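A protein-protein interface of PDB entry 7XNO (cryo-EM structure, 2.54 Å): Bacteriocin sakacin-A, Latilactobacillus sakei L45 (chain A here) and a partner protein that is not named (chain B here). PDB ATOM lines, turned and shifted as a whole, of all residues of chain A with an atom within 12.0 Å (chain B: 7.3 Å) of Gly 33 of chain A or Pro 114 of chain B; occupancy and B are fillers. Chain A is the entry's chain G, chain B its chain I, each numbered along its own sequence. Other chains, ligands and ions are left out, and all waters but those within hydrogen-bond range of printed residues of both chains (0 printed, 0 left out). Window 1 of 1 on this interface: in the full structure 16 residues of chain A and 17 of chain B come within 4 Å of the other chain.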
ATOM      1  N   GLN A  24     -36.057  -3.067   2.486  1.00  0.00           N
ATOM      2  CA  GLN A  24     -35.921  -3.644   3.819  1.00  0.00           C
ATOM      3  C   GLN A  24     -34.835  -4.711   3.847  1.00  0.00           C
ATOM      4  O   GLN A  24     -34.065  -4.796   4.809  1.00  0.00           O
ATOM      5  CB  GLN A  24     -37.257  -4.224   4.282  1.00  0.00           C
ATOM      6  CG  GLN A  24     -38.309  -3.178   4.593  1.00  0.00           C
ATOM      7  CD  GLN A  24     -37.780  -2.060   5.467  1.00  0.00           C
ATOM      8  OE1 GLN A  24     -37.565  -2.242   6.665  1.00  0.00           O
ATOM      9  NE2 GLN A  24     -37.568  -0.893   4.871  1.00  0.00           N
ATOM     10  N   SER A  25     -34.759  -5.532   2.799  1.00  0.00           N
ATOM     11  CA  SER A  25     -33.718  -6.549   2.725  1.00  0.00           C
ATOM     12  C   SER A  25     -32.336  -5.915   2.679  1.00  0.00           C
ATOM     13  O   SER A  25     -31.413  -6.375   3.360  1.00  0.00           O
ATOM     14  CB  SER A  25     -33.943  -7.442   1.506  1.00  0.00           C
ATOM     15  OG  SER A  25     -35.113  -8.225   1.661  1.00  0.00           O
ATOM     16  N   ILE A  26     -32.180  -4.849   1.892  1.00  0.00           N
ATOM     17  CA  ILE A  26     -30.890  -4.169   1.816  1.00  0.00           C
ATOM     18  C   ILE A  26     -30.508  -3.590   3.173  1.00  0.00           C
ATOM     19  O   ILE A  26     -29.364  -3.726   3.622  1.00  0.00           O
ATOM     20  CB  ILE A  26     -30.922  -3.082   0.726  1.00  0.00           C
ATOM     21  CG1 ILE A  26     -31.010  -3.723  -0.657  1.00  0.00           C
ATOM     22  CG2 ILE A  26     -29.695  -2.191   0.819  1.00  0.00           C
ATOM     23  CD1 ILE A  26     -31.256  -2.732  -1.761  1.00  0.00           C
ATOM     24  N   ILE A  27     -31.462  -2.947   3.852  1.00  0.00           N
ATOM     25  CA  ILE A  27     -31.167  -2.320   5.139  1.00  0.00           C
ATOM     26  C   ILE A  27     -30.795  -3.375   6.177  1.00  0.00           C
ATOM     27  O   ILE A  27     -29.822  -3.220   6.929  1.00  0.00           O
ATOM     28  CB  ILE A  27     -32.363  -1.467   5.601  1.00  0.00           C
ATOM     29  CG1 ILE A  27     -32.362  -0.119   4.878  1.00  0.00           C
ATOM     30  CG2 ILE A  27     -32.333  -1.262   7.108  1.00  0.00           C
ATOM     31  CD1 ILE A  27     -33.720   0.533   4.803  1.00  0.00           C
ATOM     32  N   GLY A  28     -31.564  -4.463   6.233  1.00  0.00           N
ATOM     33  CA  GLY A  28     -31.272  -5.514   7.192  1.00  0.00           C
ATOM     34  C   GLY A  28     -29.944  -6.193   6.925  1.00  0.00           C
ATOM     35  O   GLY A  28     -29.188  -6.483   7.857  1.00  0.00           O
ATOM     36  N   GLY A  29     -29.642  -6.457   5.652  1.00  0.00           N
ATOM     37  CA  GLY A  29     -28.342  -7.005   5.314  1.00  0.00           C
ATOM     38  C   GLY A  29     -27.208  -6.076   5.693  1.00  0.00           C
ATOM     39  O   GLY A  29     -26.176  -6.520   6.194  1.00  0.00           O
ATOM     40  N   MET A  30     -27.395  -4.771   5.479  1.00  0.00           N
ATOM     41  CA  MET A  30     -26.378  -3.799   5.868  1.00  0.00           C
ATOM     42  C   MET A  30     -26.123  -3.843   7.370  1.00  0.00           C
ATOM     43  O   MET A  30     -24.971  -3.920   7.815  1.00  0.00           O
ATOM     44  CB  MET A  30     -26.812  -2.397   5.442  1.00  0.00           C
ATOM     45  CG  MET A  30     -25.684  -1.389   5.355  1.00  0.00           C
ATOM     46  SD  MET A  30     -26.166   0.099   4.463  1.00  0.00           S
ATOM     47  CE  MET A  30     -27.081  -0.607   3.096  1.00  0.00           C
ATOM     48  N   ILE A  31     -27.193  -3.800   8.167  1.00  0.00           N
ATOM     49  CA  ILE A  31     -27.032  -3.772   9.620  1.00  0.00           C
ATOM     50  C   ILE A  31     -26.390  -5.064  10.111  1.00  0.00           C
ATOM     51  O   ILE A  31     -25.447  -5.044  10.916  1.00  0.00           O
ATOM     52  CB  ILE A  31     -28.383  -3.517  10.311  1.00  0.00           C
ATOM     53  CG1 ILE A  31     -28.987  -2.196   9.837  1.00  0.00           C
ATOM     54  CG2 ILE A  31     -28.210  -3.496  11.820  1.00  0.00           C
ATOM     55  CD1 ILE A  31     -30.418  -1.991  10.277  1.00  0.00           C
ATOM     56  N   SER A  32     -26.885  -6.208   9.630  1.00  0.00           N
ATOM     57  CA  SER A  32     -26.348  -7.489  10.075  1.00  0.00           C
ATOM     58  C   SER A  32     -24.895  -7.659   9.652  1.00  0.00           C
ATOM     59  O   SER A  32     -24.076  -8.165  10.426  1.00  0.00           O
ATOM     60  CB  SER A  32     -27.205  -8.635   9.536  1.00  0.00           C
ATOM     61  OG  SER A  32     -27.501  -8.451   8.164  1.00  0.00           O
ATOM     62  N   GLY A  33     -24.553  -7.235   8.434  1.00  0.00           N
ATOM     63  CA  GLY A  33     -23.178  -7.342   7.984  1.00  0.00           C
ATOM     64  C   GLY A  33     -22.236  -6.458   8.775  1.00  0.00           C
ATOM     65  O   GLY A  33     -21.141  -6.886   9.145  1.00  0.00           O
ATOM     66  N   TRP A  34     -22.650  -5.219   9.059  1.00  0.00           N
ATOM     67  CA  TRP A  34     -21.824  -4.342   9.880  1.00  0.00           C
ATOM     68  C   TRP A  34     -21.607  -4.937  11.266  1.00  0.00           C
ATOM     69  O   TRP A  34     -20.476  -4.978  11.768  1.00  0.00           O
ATOM     70  CB  TRP A  34     -22.468  -2.959   9.983  1.00  0.00           C
ATOM     71  CG  TRP A  34     -22.035  -2.014   8.908  1.00  0.00           C
ATOM     72  CD1 TRP A  34     -22.707  -1.715   7.761  1.00  0.00           C
ATOM     73  CD2 TRP A  34     -20.827  -1.243   8.877  1.00  0.00           C
ATOM     74  NE1 TRP A  34     -21.995  -0.807   7.018  1.00  0.00           N
ATOM     75  CE2 TRP A  34     -20.836  -0.502   7.681  1.00  0.00           C
ATOM     76  CE3 TRP A  34     -19.738  -1.111   9.745  1.00  0.00           C
ATOM     77  CZ2 TRP A  34     -19.801   0.360   7.330  1.00  0.00           C
ATOM     78  CZ3 TRP A  34     -18.712  -0.255   9.394  1.00  0.00           C
ATOM     79  CH2 TRP A  34     -18.751   0.471   8.198  1.00  0.00           C
ATOM     80  N   ALA A  35     -22.683  -5.424  11.888  1.00  0.00           N
ATOM     81  CA  ALA A  35     -22.570  -5.972  13.234  1.00  0.00           C
ATOM     82  C   ALA A  35     -21.691  -7.217  13.261  1.00  0.00           C
ATOM     83  O   ALA A  35     -20.847  -7.368  14.152  1.00  0.00           O
ATOM     84  CB  ALA A  35     -23.958  -6.282  13.788  1.00  0.00           C
ATOM     85  N   SER A  36     -21.864  -8.117  12.290  1.00  0.00           N
ATOM     86  CA  SER A  36     -21.081  -9.347  12.282  1.00  0.00           C
ATOM     87  C   SER A  36     -19.622  -9.077  11.940  1.00  0.00           C
ATOM     88  O   SER A  36     -18.724  -9.737  12.476  1.00  0.00           O
ATOM     89  CB  SER A  36     -21.690 -10.350  11.301  1.00  0.00           C
ATOM     90  OG  SER A  36     -21.230 -10.122   9.982  1.00  0.00           O
ATOM     91  N   GLY A  37     -19.360  -8.120  11.049  1.00  0.00           N
ATOM     92  CA  GLY A  37     -17.986  -7.776  10.731  1.00  0.00           C
ATOM     93  C   GLY A  37     -17.260  -7.133  11.895  1.00  0.00           C
ATOM     94  O   GLY A  37     -16.097  -7.448  12.161  1.00  0.00           O
ATOM     95  N   LEU A  38     -17.931  -6.224  12.607  1.00  0.00           N
ATOM     96  CA  LEU A  38     -17.280  -5.572  13.737  1.00  0.00           C
ATOM     97  C   LEU A  38     -17.164  -6.503  14.938  1.00  0.00           C
ATOM     98  O   LEU A  38     -16.219  -6.382  15.723  1.00  0.00           O
ATOM     99  CB  LEU A  38     -18.034  -4.298  14.114  1.00  0.00           C
ATOM    100  CG  LEU A  38     -17.904  -3.132  13.134  1.00  0.00           C
ATOM    101  CD1 LEU A  38     -18.694  -1.930  13.622  1.00  0.00           C
ATOM    102  CD2 LEU A  38     -16.443  -2.771  12.923  1.00  0.00           C
ATOM    103  N   ALA A  39     -18.105  -7.435  15.099  1.00  0.00           N
ATOM    104  CA  ALA A  39     -18.046  -8.376  16.209  1.00  0.00           C
ATOM    105  C   ALA A  39     -16.988  -9.453  16.018  1.00  0.00           C
ATOM    106  O   ALA A  39     -16.572 -10.074  17.002  1.00  0.00           O
ATOM    107  CB  ALA A  39     -19.412  -9.035  16.414  1.00  0.00           C
ATOM    108  N   GLY A  40     -16.546  -9.690  14.787  1.00  0.00           N
ATOM    109  CA  GLY A  40     -15.596 -10.737  14.485  1.00  0.00           C
ATOM    110  C   GLY A  40     -14.143 -10.322  14.418  1.00  0.00           C
ATOM    111  O   GLY A  40     -13.303 -11.143  14.031  1.00  0.00           O
ATOM    112  N   MET A  41     -13.811  -9.086  14.776  1.00  0.00           N
ATOM    113  CA  MET A  41     -12.423  -8.639  14.736  1.00  0.00           C
ATOM    114  C   MET A  41     -11.613  -9.276  15.861  1.00  0.00           C
ATOM    115  O   MET A  41     -12.019  -9.251  17.022  1.00  0.00           O
ATOM    116  CB  MET A  41     -12.339  -7.114  14.829  1.00  0.00           C
ATOM    117  CG  MET A  41     -13.097  -6.378  13.741  1.00  0.00           C
ATOM    118  SD  MET A  41     -13.175  -4.600  14.030  1.00  0.00           S
ATOM    119  CE  MET A  41     -13.515  -4.550  15.786  1.00  0.00           C
ATOM    120  N   HIS B  68     -10.016  -8.619   3.443  1.00  0.00           N
ATOM    121  CA  HIS B  68     -10.794  -8.166   2.301  1.00  0.00           C
ATOM    122  C   HIS B  68      -9.841  -7.794   1.170  1.00  0.00           C
ATOM    123  O   HIS B  68      -8.846  -7.097   1.409  1.00  0.00           O
ATOM    124  CB  HIS B  68     -11.664  -6.969   2.681  1.00  0.00           C
ATOM    125  CG  HIS B  68     -12.666  -6.592   1.636  1.00  0.00           C
ATOM    126  ND1 HIS B  68     -12.311  -6.018   0.435  1.00  0.00           N
ATOM    127  CD2 HIS B  68     -14.015  -6.694   1.618  1.00  0.00           C
ATOM    128  CE1 HIS B  68     -13.397  -5.794  -0.282  1.00  0.00           C
ATOM    129  NE2 HIS B  68     -14.445  -6.195   0.413  1.00  0.00           N
ATOM    130  N   LEU B 108      -9.015  -4.804   9.499  1.00  0.00           N
ATOM    131  CA  LEU B 108      -9.290  -4.274   8.168  1.00  0.00           C
ATOM    132  C   LEU B 108     -10.322  -5.122   7.439  1.00  0.00           C
ATOM    133  O   LEU B 108     -11.205  -4.582   6.768  1.00  0.00           O
ATOM    134  CB  LEU B 108      -8.000  -4.170   7.358  1.00  0.00           C
ATOM    135  CG  LEU B 108      -7.189  -2.896   7.604  1.00  0.00           C
ATOM    136  CD1 LEU B 108      -6.125  -2.721   6.540  1.00  0.00           C
ATOM    137  CD2 LEU B 108      -8.102  -1.681   7.651  1.00  0.00           C
ATOM    138  N   ALA B 109     -10.235  -6.449   7.554  1.00  0.00           N
ATOM    139  CA  ALA B 109     -11.272  -7.298   6.975  1.00  0.00           C
ATOM    140  C   ALA B 109     -12.617  -7.052   7.644  1.00  0.00           C
ATOM    141  O   ALA B 109     -13.648  -6.948   6.967  1.00  0.00           O
ATOM    142  CB  ALA B 109     -10.880  -8.770   7.089  1.00  0.00           C
ATOM    143  N   GLY B 110     -12.624  -6.940   8.975  1.00  0.00           N
ATOM    144  CA  GLY B 110     -13.861  -6.713   9.701  1.00  0.00           C
ATOM    145  C   GLY B 110     -14.511  -5.378   9.413  1.00  0.00           C
ATOM    146  O   GLY B 110     -15.721  -5.235   9.610  1.00  0.00           O
ATOM    147  N   ILE B 111     -13.732  -4.392   8.967  1.00  0.00           N
ATOM    148  CA  ILE B 111     -14.305  -3.109   8.575  1.00  0.00           C
ATOM    149  C   ILE B 111     -14.587  -3.025   7.077  1.00  0.00           C
ATOM    150  O   ILE B 111     -15.453  -2.243   6.663  1.00  0.00           O
ATOM    151  CB  ILE B 111     -13.393  -1.946   9.012  1.00  0.00           C
ATOM    152  CG1 ILE B 111     -14.167  -0.627   9.025  1.00  0.00           C
ATOM    153  CG2 ILE B 111     -12.174  -1.834   8.111  1.00  0.00           C
ATOM    154  CD1 ILE B 111     -15.195  -0.534  10.123  1.00  0.00           C
ATOM    155  N   GLY B 112     -13.899  -3.816   6.256  1.00  0.00           N
ATOM    156  CA  GLY B 112     -14.066  -3.747   4.820  1.00  0.00           C
ATOM    157  C   GLY B 112     -15.155  -4.645   4.279  1.00  0.00           C
ATOM    158  O   GLY B 112     -15.743  -4.341   3.237  1.00  0.00           O
ATOM    159  N   ASP B 113     -15.430  -5.759   4.959  1.00  0.00           N
ATOM    160  CA  ASP B 113     -16.544  -6.602   4.532  1.00  0.00           C
ATOM    161  C   ASP B 113     -17.880  -5.873   4.613  1.00  0.00           C
ATOM    162  O   ASP B 113     -18.628  -5.897   3.622  1.00  0.00           O
ATOM    163  CB  ASP B 113     -16.554  -7.909   5.335  1.00  0.00           C
ATOM    164  CG  ASP B 113     -15.532  -8.911   4.836  1.00  0.00           C
ATOM    165  OD1 ASP B 113     -14.897  -8.650   3.794  1.00  0.00           O
ATOM    166  OD2 ASP B 113     -15.363  -9.963   5.483  1.00  0.00           O
ATOM    167  N   PRO B 114     -18.248  -5.216   5.720  1.00  0.00           N
ATOM    168  CA  PRO B 114     -19.495  -4.432   5.701  1.00  0.00           C
ATOM    169  C   PRO B 114     -19.483  -3.285   4.706  1.00  0.00           C
ATOM    170  O   PRO B 114     -20.529  -2.976   4.123  1.00  0.00           O
ATOM    171  CB  PRO B 114     -19.617  -3.920   7.142  1.00  0.00           C
ATOM    172  CG  PRO B 114     -18.292  -4.120   7.760  1.00  0.00           C
ATOM    173  CD  PRO B 114     -17.671  -5.278   7.074  1.00  0.00           C
ATOM    174  N   VAL B 115     -18.334  -2.643   4.494  1.00  0.00           N
ATOM    175  CA  VAL B 115     -18.288  -1.461   3.638  1.00  0.00           C
ATOM    176  C   VAL B 115     -18.536  -1.840   2.183  1.00  0.00           C
ATOM    177  O   VAL B 115     -19.338  -1.206   1.488  1.00  0.00           O
ATOM    178  CB  VAL B 115     -16.947  -0.725   3.810  1.00  0.00           C
ATOM    179  CG1 VAL B 115     -16.668   0.167   2.612  1.00  0.00           C
ATOM    180  CG2 VAL B 115     -16.956   0.096   5.085  1.00  0.00           C
ATOM    181  N   PHE B 116     -17.862  -2.883   1.702  1.00  0.00           N
ATOM    182  CA  PHE B 116     -17.924  -3.250   0.293  1.00  0.00           C
ATOM    183  C   PHE B 116     -18.943  -4.343   0.005  1.00  0.00           C
ATOM    184  O   PHE B 116     -19.704  -4.232  -0.957  1.00  0.00           O
ATOM    185  CB  PHE B 116     -16.539  -3.686  -0.196  1.00  0.00           C
ATOM    186  CG  PHE B 116     -15.532  -2.576  -0.230  1.00  0.00           C
ATOM    187  CD1 PHE B 116     -15.698  -1.498  -1.082  1.00  0.00           C
ATOM    188  CD2 PHE B 116     -14.417  -2.609   0.590  1.00  0.00           C
ATOM    189  CE1 PHE B 116     -14.773  -0.475  -1.115  1.00  0.00           C
ATOM    190  CE2 PHE B 116     -13.489  -1.588   0.562  1.00  0.00           C
ATOM    191  CZ  PHE B 116     -13.668  -0.520  -0.291  1.00  0.00           C
ATOM    192  N   TRP B 117     -18.980  -5.399   0.817  1.00  0.00           N
ATOM    193  CA  TRP B 117     -19.872  -6.514   0.518  1.00  0.00           C
ATOM    194  C   TRP B 117     -21.321  -6.194   0.863  1.00  0.00           C
ATOM    195  O   TRP B 117     -22.237  -6.635   0.160  1.00  0.00           O
ATOM    196  CB  TRP B 117     -19.434  -7.769   1.271  1.00  0.00           C
ATOM    197  CG  TRP B 117     -18.131  -8.331   0.822  1.00  0.00           C
ATOM    198  CD1 TRP B 117     -16.916  -8.127   1.395  1.00  0.00           C
ATOM    199  CD2 TRP B 117     -17.906  -9.188  -0.300  1.00  0.00           C
ATOM    200  NE1 TRP B 117     -15.946  -8.809   0.708  1.00  0.00           N
ATOM    201  CE2 TRP B 117     -16.529  -9.466  -0.341  1.00  0.00           C
ATOM    202  CE3 TRP B 117     -18.736  -9.747  -1.277  1.00  0.00           C
ATOM    203  CZ2 TRP B 117     -15.961 -10.276  -1.313  1.00  0.00           C
ATOM    204  CZ3 TRP B 117     -18.172 -10.557  -2.238  1.00  0.00           C
ATOM    205  CH2 TRP B 117     -16.798 -10.814  -2.247  1.00  0.00           C
ATOM    206  N   PHE B 118     -21.553  -5.442   1.939  1.00  0.00           N
ATOM    207  CA  PHE B 118     -22.895  -5.274   2.473  1.00  0.00           C
ATOM    208  C   PHE B 118     -23.422  -3.847   2.436  1.00  0.00           C
ATOM    209  O   PHE B 118     -24.588  -3.637   2.788  1.00  0.00           O
ATOM    210  CB  PHE B 118     -22.956  -5.786   3.922  1.00  0.00           C
ATOM    211  CG  PHE B 118     -22.421  -7.179   4.092  1.00  0.00           C
ATOM    212  CD1 PHE B 118     -23.056  -8.256   3.501  1.00  0.00           C
ATOM    213  CD2 PHE B 118     -21.279  -7.411   4.838  1.00  0.00           C
ATOM    214  CE1 PHE B 118     -22.564  -9.536   3.652  1.00  0.00           C
ATOM    215  CE2 PHE B 118     -20.783  -8.689   4.992  1.00  0.00           C
ATOM    216  CZ  PHE B 118     -21.426  -9.753   4.399  1.00  0.00           C
ATOM    217  N   THR B 119     -22.620  -2.864   2.031  1.00  0.00           N
ATOM    218  CA  THR B 119     -23.105  -1.493   1.923  1.00  0.00           C
ATOM    219  C   THR B 119     -23.042  -0.952   0.505  1.00  0.00           C
ATOM    220  O   THR B 119     -24.059  -0.483  -0.018  1.00  0.00           O
ATOM    221  CB  THR B 119     -22.315  -0.571   2.867  1.00  0.00           C
ATOM    222  OG1 THR B 119     -22.359  -1.098   4.198  1.00  0.00           O
ATOM    223  CG2 THR B 119     -22.912   0.826   2.864  1.00  0.00           C
ATOM    224  N   VAL B 120     -21.878  -1.009  -0.141  1.00  0.00           N
ATOM    225  CA  VAL B 120     -21.732  -0.422  -1.470  1.00  0.00           C
ATOM    226  C   VAL B 120     -22.269  -1.364  -2.539  1.00  0.00           C
ATOM    227  O   VAL B 120     -23.054  -0.961  -3.408  1.00  0.00           O
ATOM    228  CB  VAL B 120     -20.257  -0.058  -1.726  1.00  0.00           C
ATOM    229  CG1 VAL B 120     -20.034   0.275  -3.190  1.00  0.00           C
ATOM    230  CG2 VAL B 120     -19.838   1.104  -0.842  1.00  0.00           C
ATOM    231  N   LYS B 121     -21.848  -2.628  -2.492  1.00  0.00           N
ATOM    232  CA  LYS B 121     -22.294  -3.597  -3.491  1.00  0.00           C
ATOM    233  C   LYS B 121     -23.803  -3.788  -3.499  1.00  0.00           C
ATOM    234  O   LYS B 121     -24.387  -3.789  -4.594  1.00  0.00           O
ATOM    235  CB  LYS B 121     -21.567  -4.930  -3.285  1.00  0.00           C
ATOM    236  CG  LYS B 121     -21.906  -5.988  -4.313  1.00  0.00           C
ATOM    237  CD  LYS B 121     -21.417  -7.354  -3.874  1.00  0.00           C
ATOM    238  CE  LYS B 121     -22.385  -8.443  -4.301  1.00  0.00           C
ATOM    239  NZ  LYS B 121     -21.901  -9.793  -3.913  1.00  0.00           N
ATOM    240  N   PRO B 122     -24.491  -3.976  -2.364  1.00  0.00           N
ATOM    241  CA  PRO B 122     -25.956  -4.106  -2.443  1.00  0.00           C
ATOM    242  C   PRO B 122     -26.642  -2.897  -3.053  1.00  0.00           C
ATOM    243  O   PRO B 122     -27.560  -3.066  -3.861  1.00  0.00           O
ATOM    244  CB  PRO B 122     -26.364  -4.315  -0.979  1.00  0.00           C
ATOM    245  CG  PRO B 122     -25.170  -4.901  -0.347  1.00  0.00           C
ATOM    246  CD  PRO B 122     -24.012  -4.206  -0.990  1.00  0.00           C
ATOM    247  N   ILE B 192     -30.241  -7.667  16.245  1.00  0.00           N
ATOM    248  CA  ILE B 192     -30.697  -7.607  14.862  1.00  0.00           C
ATOM    249  C   ILE B 192     -30.849  -9.003  14.272  1.00  0.00           C
ATOM    250  O   ILE B 192     -31.716  -9.227  13.425  1.00  0.00           O
ATOM    251  CB  ILE B 192     -29.760  -6.718  14.020  1.00  0.00           C
ATOM    252  CG1 ILE B 192     -30.490  -6.216  12.775  1.00  0.00           C
ATOM    253  CG2 ILE B 192     -28.484  -7.453  13.637  1.00  0.00           C
ATOM    254  CD1 ILE B 192     -31.661  -5.308  13.084  1.00  0.00           C
ATOM    255  N   LEU B 193     -30.034  -9.968  14.706  1.00  0.00           N
ATOM    256  CA  LEU B 193     -30.185 -11.334  14.227  1.00  0.00           C
ATOM    257  C   LEU B 193     -31.425 -11.994  14.803  1.00  0.00           C
ATOM    258  O   LEU B 193     -32.066 -12.790  14.116  1.00  0.00           O
ATOM    259  CB  LEU B 193     -28.938 -12.157  14.550  1.00  0.00           C
ATOM    260  CG  LEU B 193     -27.872 -12.273  13.454  1.00  0.00           C
ATOM    261  CD1 LEU B 193     -28.419 -13.050  12.268  1.00  0.00           C
ATOM    262  CD2 LEU B 193     -27.368 -10.913  13.002  1.00  0.00           C
ATOM    263  N   LEU B 196     -34.073 -10.585  12.558  1.00  0.00           N
ATOM    264  CA  LEU B 196     -34.031 -11.190  11.231  1.00  0.00           C
ATOM    265  C   LEU B 196     -34.497 -12.639  11.249  1.00  0.00           C
ATOM    266  O   LEU B 196     -35.118 -13.094  10.286  1.00  0.00           O
ATOM    267  CB  LEU B 196     -32.620 -11.098  10.651  1.00  0.00           C
ATOM    268  CG  LEU B 196     -32.104  -9.700  10.306  1.00  0.00           C
ATOM    269  CD1 LEU B 196     -30.756  -9.787   9.618  1.00  0.00           C
ATOM    270  CD2 LEU B 196     -33.103  -8.952   9.440  1.00  0.00           C
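Of the 18 printed residues of chain A, 7 touch a printed residue of chain B. Hydrophobic or aromatic side chains of chain B within 4 Å of the printed part of chain A: Ile 111, Pro 114, Val 115, Phe 118, Ile 192 and Leu 196. Among the printed residues, 13 pairs touch across the chains. Among the printed residues, no Asp or Glu carboxylate lies within 4 Å of a Lys or Arg side-chain nitrogen of the other chain.
NE1 of Trp 34 of chain A lies within hydrogen-bond range of OG1 of Thr 119 of chain B, 2.9 Å away. The backbone carbonyl oxygen (O) of Gly 37 of chain A lies close to the backbone carbonyl oxygen (O) of Gly 110 of chain B (3.4 Å).
Of the printed residues of chain B, Met 30 of chain A touches Phe 118 and Thr 119. Of the printed residues of chain B, Ile 31 of chain A touches Ile 192. Gly 33 of chain A touches just these residues of chain B: Pro 114 (3.9 Å) and Phe 118 (3.7 Å). Of the printed residues of chain B, Trp 34 of chain A touches Ile 111, Pro 114, Val 115 and Thr 119. No residue of chain A comes within 4 Å of Ala 109 of chain B. Of chain A, only Gly 37 (3.3 Å) and Leu 38 (3.9 Å) come within 4 Å of Gly 110 of chain B. Ile 111 of chain B touches just these residues of chain A: Trp 34 (3.6 Å) and Leu 38 (3.8 Å). No residue of chain A comes within 4 Å of Gly 112 of chain B. Of chain A, only Gly 33 and Trp 34 come within 4 Å of Pro 114 of chain B. Of the printed residues of chain A, Phe 118 of chain B touches Met 30 (3.6 Å) and Gly 33 (3.7 Å). Printed residues of chain A within 4 Å of Thr 119 of chain B: Met 30 (3.5 Å) and Trp 34 (2.9 Å).
OG1 of Thr 119 of chain B touches CG of Met 30 of chain A, 3.5 Å away. CG2 of Ile 31 of chain A touches CG1 of Ile 192 of chain B (3.7 Å). Leu 196 of chain B touches Ser 32 of chain A (CD1 to CB, 3.7 Å). Gly 33 of chain A touches Pro 114 of chain B. Phe 118 of chain B touches Gly 33 of chain A. Ile 111 of chain B touches Trp 34 of chain A (CD1 to CZ3, 3.6 Å). Pro 114 of chain B touches Trp 34 of chain A (CB to CD2, 3.4 Å). CH2 of Trp 34 of chain A touches CG2 of Val 115 of chain B, 3.6 Å away. Gly 110 of chain B touches Leu 38 of chain A. Leu 38 of chain A touches Ile 111 of chain B.
The backbone carbonyl oxygen (O) of Gly 33 of chain A lies within hydrogen-bond range of the side-chain hydroxyl (OG) of Ser 36 of chain A. The side-chain hydroxyl of Ser 36 of chain A lies close to the backbone carbonyl oxygen of Ser 32 of chain A. The backbone carbonyl oxygen (O) of Gly 28 of chain A sits at hydrogen-bond distance from the side-chain hydroxyl (OG) of Ser 32 of chain A (2.6 Å). The backbone carbonyl oxygen (O) of Val 115 of chain B is in hydrogen-bond range of the backbone NH (N) of Val 120 of chain B. O of Pro 114 of chain B lies within hydrogen-bond range of OG1 of Thr 119 of chain B, at 2.6 Å. N of Phe 118 of chain B sits close to O of Asp 113 of chain B.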
